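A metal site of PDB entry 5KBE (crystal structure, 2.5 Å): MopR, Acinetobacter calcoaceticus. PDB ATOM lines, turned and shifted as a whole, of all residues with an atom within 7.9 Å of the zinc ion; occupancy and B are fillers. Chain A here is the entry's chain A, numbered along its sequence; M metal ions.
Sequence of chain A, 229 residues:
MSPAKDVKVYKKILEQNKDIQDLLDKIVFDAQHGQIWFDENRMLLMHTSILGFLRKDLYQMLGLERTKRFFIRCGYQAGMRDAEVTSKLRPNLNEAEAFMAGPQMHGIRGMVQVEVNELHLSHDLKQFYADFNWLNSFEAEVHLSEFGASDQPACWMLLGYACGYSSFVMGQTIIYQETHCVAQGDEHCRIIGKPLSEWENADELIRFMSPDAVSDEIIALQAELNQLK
SG of Cys 189 binds the zinc ion (2.2 Å). The side-chain sulfur (SG) of Cys 181 is bound to the zinc ion, at 2.3 Å. The side-chain carboxylate (OE2) of Glu 178 is bound to the zinc ion (2.3 Å). SG of Cys 155 is bound to the zinc ion.
Residues that only touch the zinc ion: Ala 140 and Val 182. Within 4 Å of the zinc ion: Ala 140, Cys 155, Glu 178, Cys 181, Val 182 and Cys 189.
The backbone carbonyl oxygen of Cys 189 is in hydrogen-bond range of the backbone NH of Trp 134, 2.8 Å away. The backbone NH (N) of Val 182 lies close to the side-chain sulfur (SG) of Cys 189. N of Ala 154 lies close to SG of Cys 181 (3.3 Å). The side-chain sulfur of Cys 155 lies close to the side-chain hydroxyl of Ser 137 (3.0 Å). SG of Cys 181 lies close to N of Ala 183. N of Cys 181 is in hydrogen-bond range of OD2 of Asp 186, at 3.0 Å. OG of Ser 137 sits at hydrogen-bond distance from N of Ala 140 (3.1 Å). The side-chain sulfur (SG) of Cys 155 lies close to the backbone NH (N) of Ala 140 (3.6 Å).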
ATOM      1  N   VAL A 112      -6.579 -19.748  -5.216  1.00  0.00           N
ATOM      2  CA  VAL A 112      -5.331 -20.187  -4.636  1.00  0.00           C
ATOM      3  C   VAL A 112      -5.561 -21.403  -3.707  1.00  0.00           C
ATOM      4  O   VAL A 112      -6.656 -21.617  -3.185  1.00  0.00           O
ATOM      5  CB  VAL A 112      -4.622 -18.989  -3.930  1.00  0.00           C
ATOM      6  CG1 VAL A 112      -5.296 -18.677  -2.582  1.00  0.00           C
ATOM      7  CG2 VAL A 112      -3.138 -19.256  -3.741  1.00  0.00           C
ATOM      8  N   TRP A 134       0.800 -20.172  -0.338  1.00  0.00           N
ATOM      9  CA  TRP A 134      -0.178 -20.019  -1.368  1.00  0.00           C
ATOM     10  C   TRP A 134       0.360 -20.714  -2.567  1.00  0.00           C
ATOM     11  O   TRP A 134       1.393 -20.305  -3.147  1.00  0.00           O
ATOM     12  CB  TRP A 134      -0.380 -18.534  -1.677  1.00  0.00           C
ATOM     13  CG  TRP A 134      -1.498 -17.800  -0.907  1.00  0.00           C
ATOM     14  CD1 TRP A 134      -2.538 -18.331  -0.157  1.00  0.00           C
ATOM     15  CD2 TRP A 134      -1.704 -16.300  -0.876  1.00  0.00           C
ATOM     16  NE1 TRP A 134      -3.348 -17.288   0.321  1.00  0.00           N
ATOM     17  CE2 TRP A 134      -2.893 -16.062  -0.081  1.00  0.00           C
ATOM     18  CE3 TRP A 134      -1.042 -15.203  -1.464  1.00  0.00           C
ATOM     19  CZ2 TRP A 134      -3.368 -14.779   0.148  1.00  0.00           C
ATOM     20  CZ3 TRP A 134      -1.499 -13.910  -1.198  1.00  0.00           C
ATOM     21  CH2 TRP A 134      -2.652 -13.696  -0.420  1.00  0.00           C
ATOM     22  N   SER A 137      -1.290 -19.608  -7.155  1.00  0.00           N
ATOM     23  CA  SER A 137      -2.024 -18.370  -7.155  1.00  0.00           C
ATOM     24  C   SER A 137      -2.364 -17.955  -8.604  1.00  0.00           C
ATOM     25  O   SER A 137      -1.499 -17.934  -9.488  1.00  0.00           O
ATOM     26  CB  SER A 137      -1.206 -17.294  -6.439  1.00  0.00           C
ATOM     27  OG  SER A 137      -1.523 -16.071  -7.038  1.00  0.00           O
ATOM     28  N   PHE A 138      -3.629 -17.662  -8.880  1.00  0.00           N
ATOM     29  CA  PHE A 138      -3.996 -17.280 -10.230  1.00  0.00           C
ATOM     30  C   PHE A 138      -3.491 -15.885 -10.550  1.00  0.00           C
ATOM     31  O   PHE A 138      -3.375 -15.471 -11.713  1.00  0.00           O
ATOM     32  CB  PHE A 138      -5.516 -17.290 -10.387  1.00  0.00           C
ATOM     33  CG  PHE A 138      -6.135 -15.979 -10.053  1.00  0.00           C
ATOM     34  CD1 PHE A 138      -6.186 -14.968 -11.006  1.00  0.00           C
ATOM     35  CD2 PHE A 138      -6.588 -15.731  -8.773  1.00  0.00           C
ATOM     36  CE1 PHE A 138      -6.723 -13.716 -10.689  1.00  0.00           C
ATOM     37  CE2 PHE A 138      -7.102 -14.511  -8.438  1.00  0.00           C
ATOM     38  CZ  PHE A 138      -7.178 -13.498  -9.408  1.00  0.00           C
ATOM     39  N   GLU A 139      -3.227 -15.113  -9.511  1.00  0.00           N
ATOM     40  CA  GLU A 139      -2.979 -13.696  -9.672  1.00  0.00           C
ATOM     41  C   GLU A 139      -1.494 -13.472 -10.021  1.00  0.00           C
ATOM     42  O   GLU A 139      -1.140 -12.562 -10.765  1.00  0.00           O
ATOM     43  CB  GLU A 139      -3.370 -13.001  -8.374  1.00  0.00           C
ATOM     44  CG  GLU A 139      -3.597 -11.516  -8.507  1.00  0.00           C
ATOM     45  CD  GLU A 139      -4.340 -10.871  -7.298  1.00  0.00           C
ATOM     46  OE1 GLU A 139      -4.442 -11.530  -6.221  1.00  0.00           O
ATOM     47  OE2 GLU A 139      -4.775  -9.666  -7.402  1.00  0.00           O
ATOM     48  N   ALA A 140      -0.616 -14.309  -9.464  1.00  0.00           N
ATOM     49  CA  ALA A 140       0.795 -14.300  -9.838  1.00  0.00           C
ATOM     50  C   ALA A 140       0.926 -14.686 -11.313  1.00  0.00           C
ATOM     51  O   ALA A 140       1.635 -14.021 -12.046  1.00  0.00           O
ATOM     52  CB  ALA A 140       1.629 -15.229  -8.940  1.00  0.00           C
ATOM     53  N   GLU A 141       0.221 -15.741 -11.721  1.00  0.00           N
ATOM     54  CA  GLU A 141       0.191 -16.168 -13.132  1.00  0.00           C
ATOM     55  C   GLU A 141      -0.213 -14.979 -14.022  1.00  0.00           C
ATOM     56  O   GLU A 141       0.531 -14.617 -14.949  1.00  0.00           O
ATOM     57  CB  GLU A 141      -0.818 -17.304 -13.294  1.00  0.00           C
ATOM     58  CG  GLU A 141      -0.351 -18.613 -13.943  1.00  0.00           C
ATOM     59  CD  GLU A 141      -1.209 -19.829 -13.510  1.00  0.00           C
ATOM     60  OE1 GLU A 141      -2.413 -19.908 -13.874  1.00  0.00           O
ATOM     61  OE2 GLU A 141      -0.696 -20.713 -12.774  1.00  0.00           O
ATOM     62  N   HIS A 143      -0.358 -11.894 -13.440  1.00  0.00           N
ATOM     63  CA  HIS A 143       0.586 -10.796 -13.367  1.00  0.00           C
ATOM     64  C   HIS A 143       1.854 -10.974 -14.186  1.00  0.00           C
ATOM     65  O   HIS A 143       2.281 -10.027 -14.847  1.00  0.00           O
ATOM     66  CB  HIS A 143       0.907 -10.436 -11.938  1.00  0.00           C
ATOM     67  CG  HIS A 143       1.704  -9.172 -11.817  1.00  0.00           C
ATOM     68  ND1 HIS A 143       1.131  -7.989 -11.564  1.00  0.00           N
ATOM     69  CD2 HIS A 143       3.077  -8.919 -11.957  1.00  0.00           C
ATOM     70  CE1 HIS A 143       2.067  -7.013 -11.528  1.00  0.00           C
ATOM     71  NE2 HIS A 143       3.261  -7.581 -11.773  1.00  0.00           N
ATOM     72  N   GLN A 152       7.806  -6.436  -6.722  1.00  0.00           N
ATOM     73  CA  GLN A 152       7.003  -6.509  -5.517  1.00  0.00           C
ATOM     74  C   GLN A 152       5.976  -7.669  -5.602  1.00  0.00           C
ATOM     75  O   GLN A 152       5.700  -8.192  -6.712  1.00  0.00           O
ATOM     76  CB  GLN A 152       6.279  -5.194  -5.343  1.00  0.00           C
ATOM     77  CG  GLN A 152       5.400  -4.917  -6.539  1.00  0.00           C
ATOM     78  CD  GLN A 152       4.766  -3.546  -6.487  1.00  0.00           C
ATOM     79  OE1 GLN A 152       3.735  -3.337  -5.796  1.00  0.00           O
ATOM     80  NE2 GLN A 152       5.366  -2.610  -7.237  1.00  0.00           N
ATOM     81  N   PRO A 153       5.457  -8.114  -4.435  1.00  0.00           N
ATOM     82  CA  PRO A 153       4.425  -9.152  -4.498  1.00  0.00           C
ATOM     83  C   PRO A 153       3.233  -8.689  -5.330  1.00  0.00           C
ATOM     84  O   PRO A 153       2.938  -7.515  -5.355  1.00  0.00           O
ATOM     85  CB  PRO A 153       4.064  -9.378  -3.014  1.00  0.00           C
ATOM     86  CG  PRO A 153       4.663  -8.259  -2.272  1.00  0.00           C
ATOM     87  CD  PRO A 153       5.836  -7.792  -3.055  1.00  0.00           C
ATOM     88  N   ALA A 154       2.571  -9.599  -6.025  1.00  0.00           N
ATOM     89  CA  ALA A 154       1.567  -9.252  -7.052  1.00  0.00           C
ATOM     90  C   ALA A 154       0.102  -9.586  -6.647  1.00  0.00           C
ATOM     91  O   ALA A 154      -0.868  -9.178  -7.325  1.00  0.00           O
ATOM     92  CB  ALA A 154       1.862 -10.038  -8.328  1.00  0.00           C
ATOM     93  N   CYS A 155      -0.024 -10.395  -5.607  1.00  0.00           N
ATOM     94  CA  CYS A 155      -1.274 -11.065  -5.298  1.00  0.00           C
ATOM     95  C   CYS A 155      -2.216 -10.184  -4.447  1.00  0.00           C
ATOM     96  O   CYS A 155      -2.644 -10.580  -3.353  1.00  0.00           O
ATOM     97  CB  CYS A 155      -1.016 -12.453  -4.697  1.00  0.00           C
ATOM     98  SG  CYS A 155      -0.246 -13.584  -5.908  1.00  0.00           S
ATOM     99  N   TRP A 156      -2.512  -8.992  -5.000  1.00  0.00           N
ATOM    100  CA  TRP A 156      -3.307  -7.973  -4.341  1.00  0.00           C
ATOM    101  C   TRP A 156      -4.710  -8.402  -3.924  1.00  0.00           C
ATOM    102  O   TRP A 156      -5.089  -8.228  -2.797  1.00  0.00           O
ATOM    103  CB  TRP A 156      -3.445  -6.790  -5.255  1.00  0.00           C
ATOM    104  CG  TRP A 156      -2.140  -6.347  -5.810  1.00  0.00           C
ATOM    105  CD1 TRP A 156      -0.911  -6.431  -5.200  1.00  0.00           C
ATOM    106  CD2 TRP A 156      -1.884  -5.763  -7.131  1.00  0.00           C
ATOM    107  NE1 TRP A 156       0.078  -5.928  -6.025  1.00  0.00           N
ATOM    108  CE2 TRP A 156      -0.441  -5.514  -7.200  1.00  0.00           C
ATOM    109  CE3 TRP A 156      -2.682  -5.419  -8.223  1.00  0.00           C
ATOM    110  CZ2 TRP A 156       0.173  -4.926  -8.322  1.00  0.00           C
ATOM    111  CZ3 TRP A 156      -2.050  -4.803  -9.359  1.00  0.00           C
ATOM    112  CH2 TRP A 156      -0.668  -4.567  -9.391  1.00  0.00           C
ATOM    113  N   LEU A 158      -6.068 -11.528  -3.685  1.00  0.00           N
ATOM    114  CA  LEU A 158      -5.955 -12.626  -2.722  1.00  0.00           C
ATOM    115  C   LEU A 158      -5.655 -12.074  -1.333  1.00  0.00           C
ATOM    116  O   LEU A 158      -6.191 -12.584  -0.335  1.00  0.00           O
ATOM    117  CB  LEU A 158      -4.856 -13.603  -3.111  1.00  0.00           C
ATOM    118  CG  LEU A 158      -4.974 -14.203  -4.508  1.00  0.00           C
ATOM    119  CD1 LEU A 158      -3.850 -15.189  -4.802  1.00  0.00           C
ATOM    120  CD2 LEU A 158      -6.318 -14.871  -4.614  1.00  0.00           C
ATOM    121  N   GLU A 178       2.390 -10.253   2.030  1.00  0.00           N
ATOM    122  CA  GLU A 178       2.831 -11.299   1.103  1.00  0.00           C
ATOM    123  C   GLU A 178       4.344 -11.277   1.059  1.00  0.00           C
ATOM    124  O   GLU A 178       5.007 -10.432   0.448  1.00  0.00           O
ATOM    125  CB  GLU A 178       2.154 -11.231  -0.291  1.00  0.00           C
ATOM    126  CG  GLU A 178       2.636 -12.379  -1.152  1.00  0.00           C
ATOM    127  CD  GLU A 178       2.021 -12.488  -2.552  1.00  0.00           C
ATOM    128  OE1 GLU A 178       1.561 -11.451  -3.106  1.00  0.00           O
ATOM    129  OE2 GLU A 178       2.074 -13.612  -3.101  1.00  0.00           O
ATOM    130  N   THR A 179       4.898 -12.279   1.706  1.00  0.00           N
ATOM    131  CA  THR A 179       6.278 -12.308   2.078  1.00  0.00           C
ATOM    132  C   THR A 179       7.182 -12.824   0.949  1.00  0.00           C
ATOM    133  O   THR A 179       8.386 -12.598   0.971  1.00  0.00           O
ATOM    134  CB  THR A 179       6.267 -13.211   3.304  1.00  0.00           C
ATOM    135  OG1 THR A 179       6.723 -12.484   4.444  1.00  0.00           O
ATOM    136  CG2 THR A 179       6.963 -14.523   3.127  1.00  0.00           C
ATOM    137  N   HIS A 180       6.603 -13.522  -0.012  1.00  0.00           N
ATOM    138  CA  HIS A 180       7.306 -14.275  -0.999  1.00  0.00           C
ATOM    139  C   HIS A 180       6.268 -14.398  -2.042  1.00  0.00           C
ATOM    140  O   HIS A 180       5.096 -14.692  -1.680  1.00  0.00           O
ATOM    141  CB  HIS A 180       7.646 -15.664  -0.489  1.00  0.00           C
ATOM    142  CG  HIS A 180       8.872 -15.696   0.395  1.00  0.00           C
ATOM    143  ND1 HIS A 180       8.832 -16.082   1.677  1.00  0.00           N
ATOM    144  CD2 HIS A 180      10.183 -15.311   0.142  1.00  0.00           C
ATOM    145  CE1 HIS A 180      10.050 -15.977   2.212  1.00  0.00           C
ATOM    146  NE2 HIS A 180      10.876 -15.503   1.273  1.00  0.00           N
ATOM    147  N   CYS A 181       6.616 -14.133  -3.309  1.00  0.00           N
ATOM    148  CA  CYS A 181       5.597 -14.176  -4.325  1.00  0.00           C
ATOM    149  C   CYS A 181       6.116 -14.843  -5.599  1.00  0.00           C
ATOM    150  O   CYS A 181       7.227 -14.597  -6.042  1.00  0.00           O
ATOM    151  CB  CYS A 181       5.028 -12.755  -4.596  1.00  0.00           C
ATOM    152  SG  CYS A 181       3.645 -12.711  -5.817  1.00  0.00           S
ATOM    153  N   VAL A 182       5.308 -15.695  -6.211  1.00  0.00           N
ATOM    154  CA  VAL A 182       5.693 -16.316  -7.451  1.00  0.00           C
ATOM    155  C   VAL A 182       6.092 -15.262  -8.497  1.00  0.00           C
ATOM    156  O   VAL A 182       6.986 -15.512  -9.285  1.00  0.00           O
ATOM    157  CB  VAL A 182       4.574 -17.233  -7.941  1.00  0.00           C
ATOM    158  CG1 VAL A 182       4.654 -17.463  -9.409  1.00  0.00           C
ATOM    159  CG2 VAL A 182       4.593 -18.572  -7.195  1.00  0.00           C
ATOM    160  N   ALA A 183       5.490 -14.068  -8.503  1.00  0.00           N
ATOM    161  CA  ALA A 183       5.804 -13.096  -9.561  1.00  0.00           C
ATOM    162  C   ALA A 183       7.140 -12.333  -9.368  1.00  0.00           C
ATOM    163  O   ALA A 183       7.530 -11.479 -10.170  1.00  0.00           O
ATOM    164  CB  ALA A 183       4.674 -12.107  -9.687  1.00  0.00           C
ATOM    165  N   GLN A 184       7.794 -12.582  -8.259  1.00  0.00           N
ATOM    166  CA  GLN A 184       9.047 -11.967  -7.953  1.00  0.00           C
ATOM    167  C   GLN A 184      10.063 -13.076  -8.074  1.00  0.00           C
ATOM    168  O   GLN A 184      11.153 -12.930  -7.575  1.00  0.00           O
ATOM    169  CB  GLN A 184       9.056 -11.496  -6.511  1.00  0.00           C
ATOM    170  CG  GLN A 184       8.199 -10.296  -6.258  1.00  0.00           C
ATOM    171  CD  GLN A 184       8.302  -9.824  -4.828  1.00  0.00           C
ATOM    172  OE1 GLN A 184       7.553 -10.278  -3.940  1.00  0.00           O
ATOM    173  NE2 GLN A 184       9.220  -8.888  -4.586  1.00  0.00           N
ATOM    174  N   ASP A 186       9.951 -16.041  -6.610  1.00  0.00           N
ATOM    175  CA  ASP A 186       9.856 -17.045  -5.565  1.00  0.00           C
ATOM    176  C   ASP A 186       9.157 -18.284  -6.061  1.00  0.00           C
ATOM    177  O   ASP A 186       8.495 -18.284  -7.109  1.00  0.00           O
ATOM    178  CB  ASP A 186       9.236 -16.480  -4.303  1.00  0.00           C
ATOM    179  CG  ASP A 186      10.086 -15.400  -3.691  1.00  0.00           C
ATOM    180  OD1 ASP A 186      11.292 -15.707  -3.407  1.00  0.00           O
ATOM    181  OD2 ASP A 186       9.597 -14.250  -3.520  1.00  0.00           O
ATOM    182  N   HIS A 188       6.948 -20.570  -4.285  1.00  0.00           N
ATOM    183  CA  HIS A 188       5.539 -20.492  -3.987  1.00  0.00           C
ATOM    184  C   HIS A 188       5.329 -19.110  -3.402  1.00  0.00           C
ATOM    185  O   HIS A 188       6.288 -18.361  -3.239  1.00  0.00           O
ATOM    186  CB  HIS A 188       5.093 -21.647  -3.061  1.00  0.00           C
ATOM    187  CG  HIS A 188       5.912 -21.773  -1.772  1.00  0.00           C
ATOM    188  ND1 HIS A 188       5.784 -20.913  -0.733  1.00  0.00           N
ATOM    189  CD2 HIS A 188       6.910 -22.690  -1.406  1.00  0.00           C
ATOM    190  CE1 HIS A 188       6.633 -21.266   0.266  1.00  0.00           C
ATOM    191  NE2 HIS A 188       7.333 -22.347  -0.150  1.00  0.00           N
ATOM    192  N   CYS A 189       4.060 -18.735  -3.156  1.00  0.00           N
ATOM    193  CA  CYS A 189       3.695 -17.476  -2.502  1.00  0.00           C
ATOM    194  C   CYS A 189       3.553 -17.781  -0.992  1.00  0.00           C
ATOM    195  O   CYS A 189       3.240 -18.902  -0.624  1.00  0.00           O
ATOM    196  CB  CYS A 189       2.372 -16.849  -3.092  1.00  0.00           C
ATOM    197  SG  CYS A 189       2.382 -16.238  -4.844  1.00  0.00           S
ATOM    198  N   ARG A 190       3.798 -16.804  -0.136  1.00  0.00           N
ATOM    199  CA  ARG A 190       3.603 -17.029   1.265  1.00  0.00           C
ATOM    200  C   ARG A 190       3.180 -15.714   1.918  1.00  0.00           C
ATOM    201  O   ARG A 190       3.716 -14.644   1.560  1.00  0.00           O
ATOM    202  CB  ARG A 190       4.892 -17.541   1.874  1.00  0.00           C
ATOM    203  CG  ARG A 190       4.959 -17.364   3.387  1.00  0.00           C
ATOM    204  CD  ARG A 190       5.889 -18.396   3.959  1.00  0.00           C
ATOM    205  NE  ARG A 190       6.316 -17.951   5.266  1.00  0.00           N
ATOM    206  CZ  ARG A 190       7.297 -18.499   5.982  1.00  0.00           C
ATOM    207  NH1 ARG A 190       8.001 -19.553   5.486  1.00  0.00           N
ATOM    208  NH2 ARG A 190       7.571 -17.963   7.198  1.00  0.00           N
ATOM    209  N   ILE A 191       2.237 -15.804   2.875  1.00  0.00           N
ATOM    210  CA  ILE A 191       1.740 -14.678   3.643  1.00  0.00           C
ATOM    211  C   ILE A 191       1.843 -14.887   5.151  1.00  0.00           C
ATOM    212  O   ILE A 191       1.882 -16.007   5.632  1.00  0.00           O
ATOM    213  CB  ILE A 191       0.248 -14.444   3.370  1.00  0.00           C
ATOM    214  CG1 ILE A 191      -0.609 -15.628   3.830  1.00  0.00           C
ATOM    215  CG2 ILE A 191      -0.023 -14.227   1.909  1.00  0.00           C
ATOM    216  CD1 ILE A 191      -2.077 -15.471   3.470  1.00  0.00           C
HETATM  217 ZN    ZN M   1       1.930 -14.092  -5.311  1.00  0.00          ZN
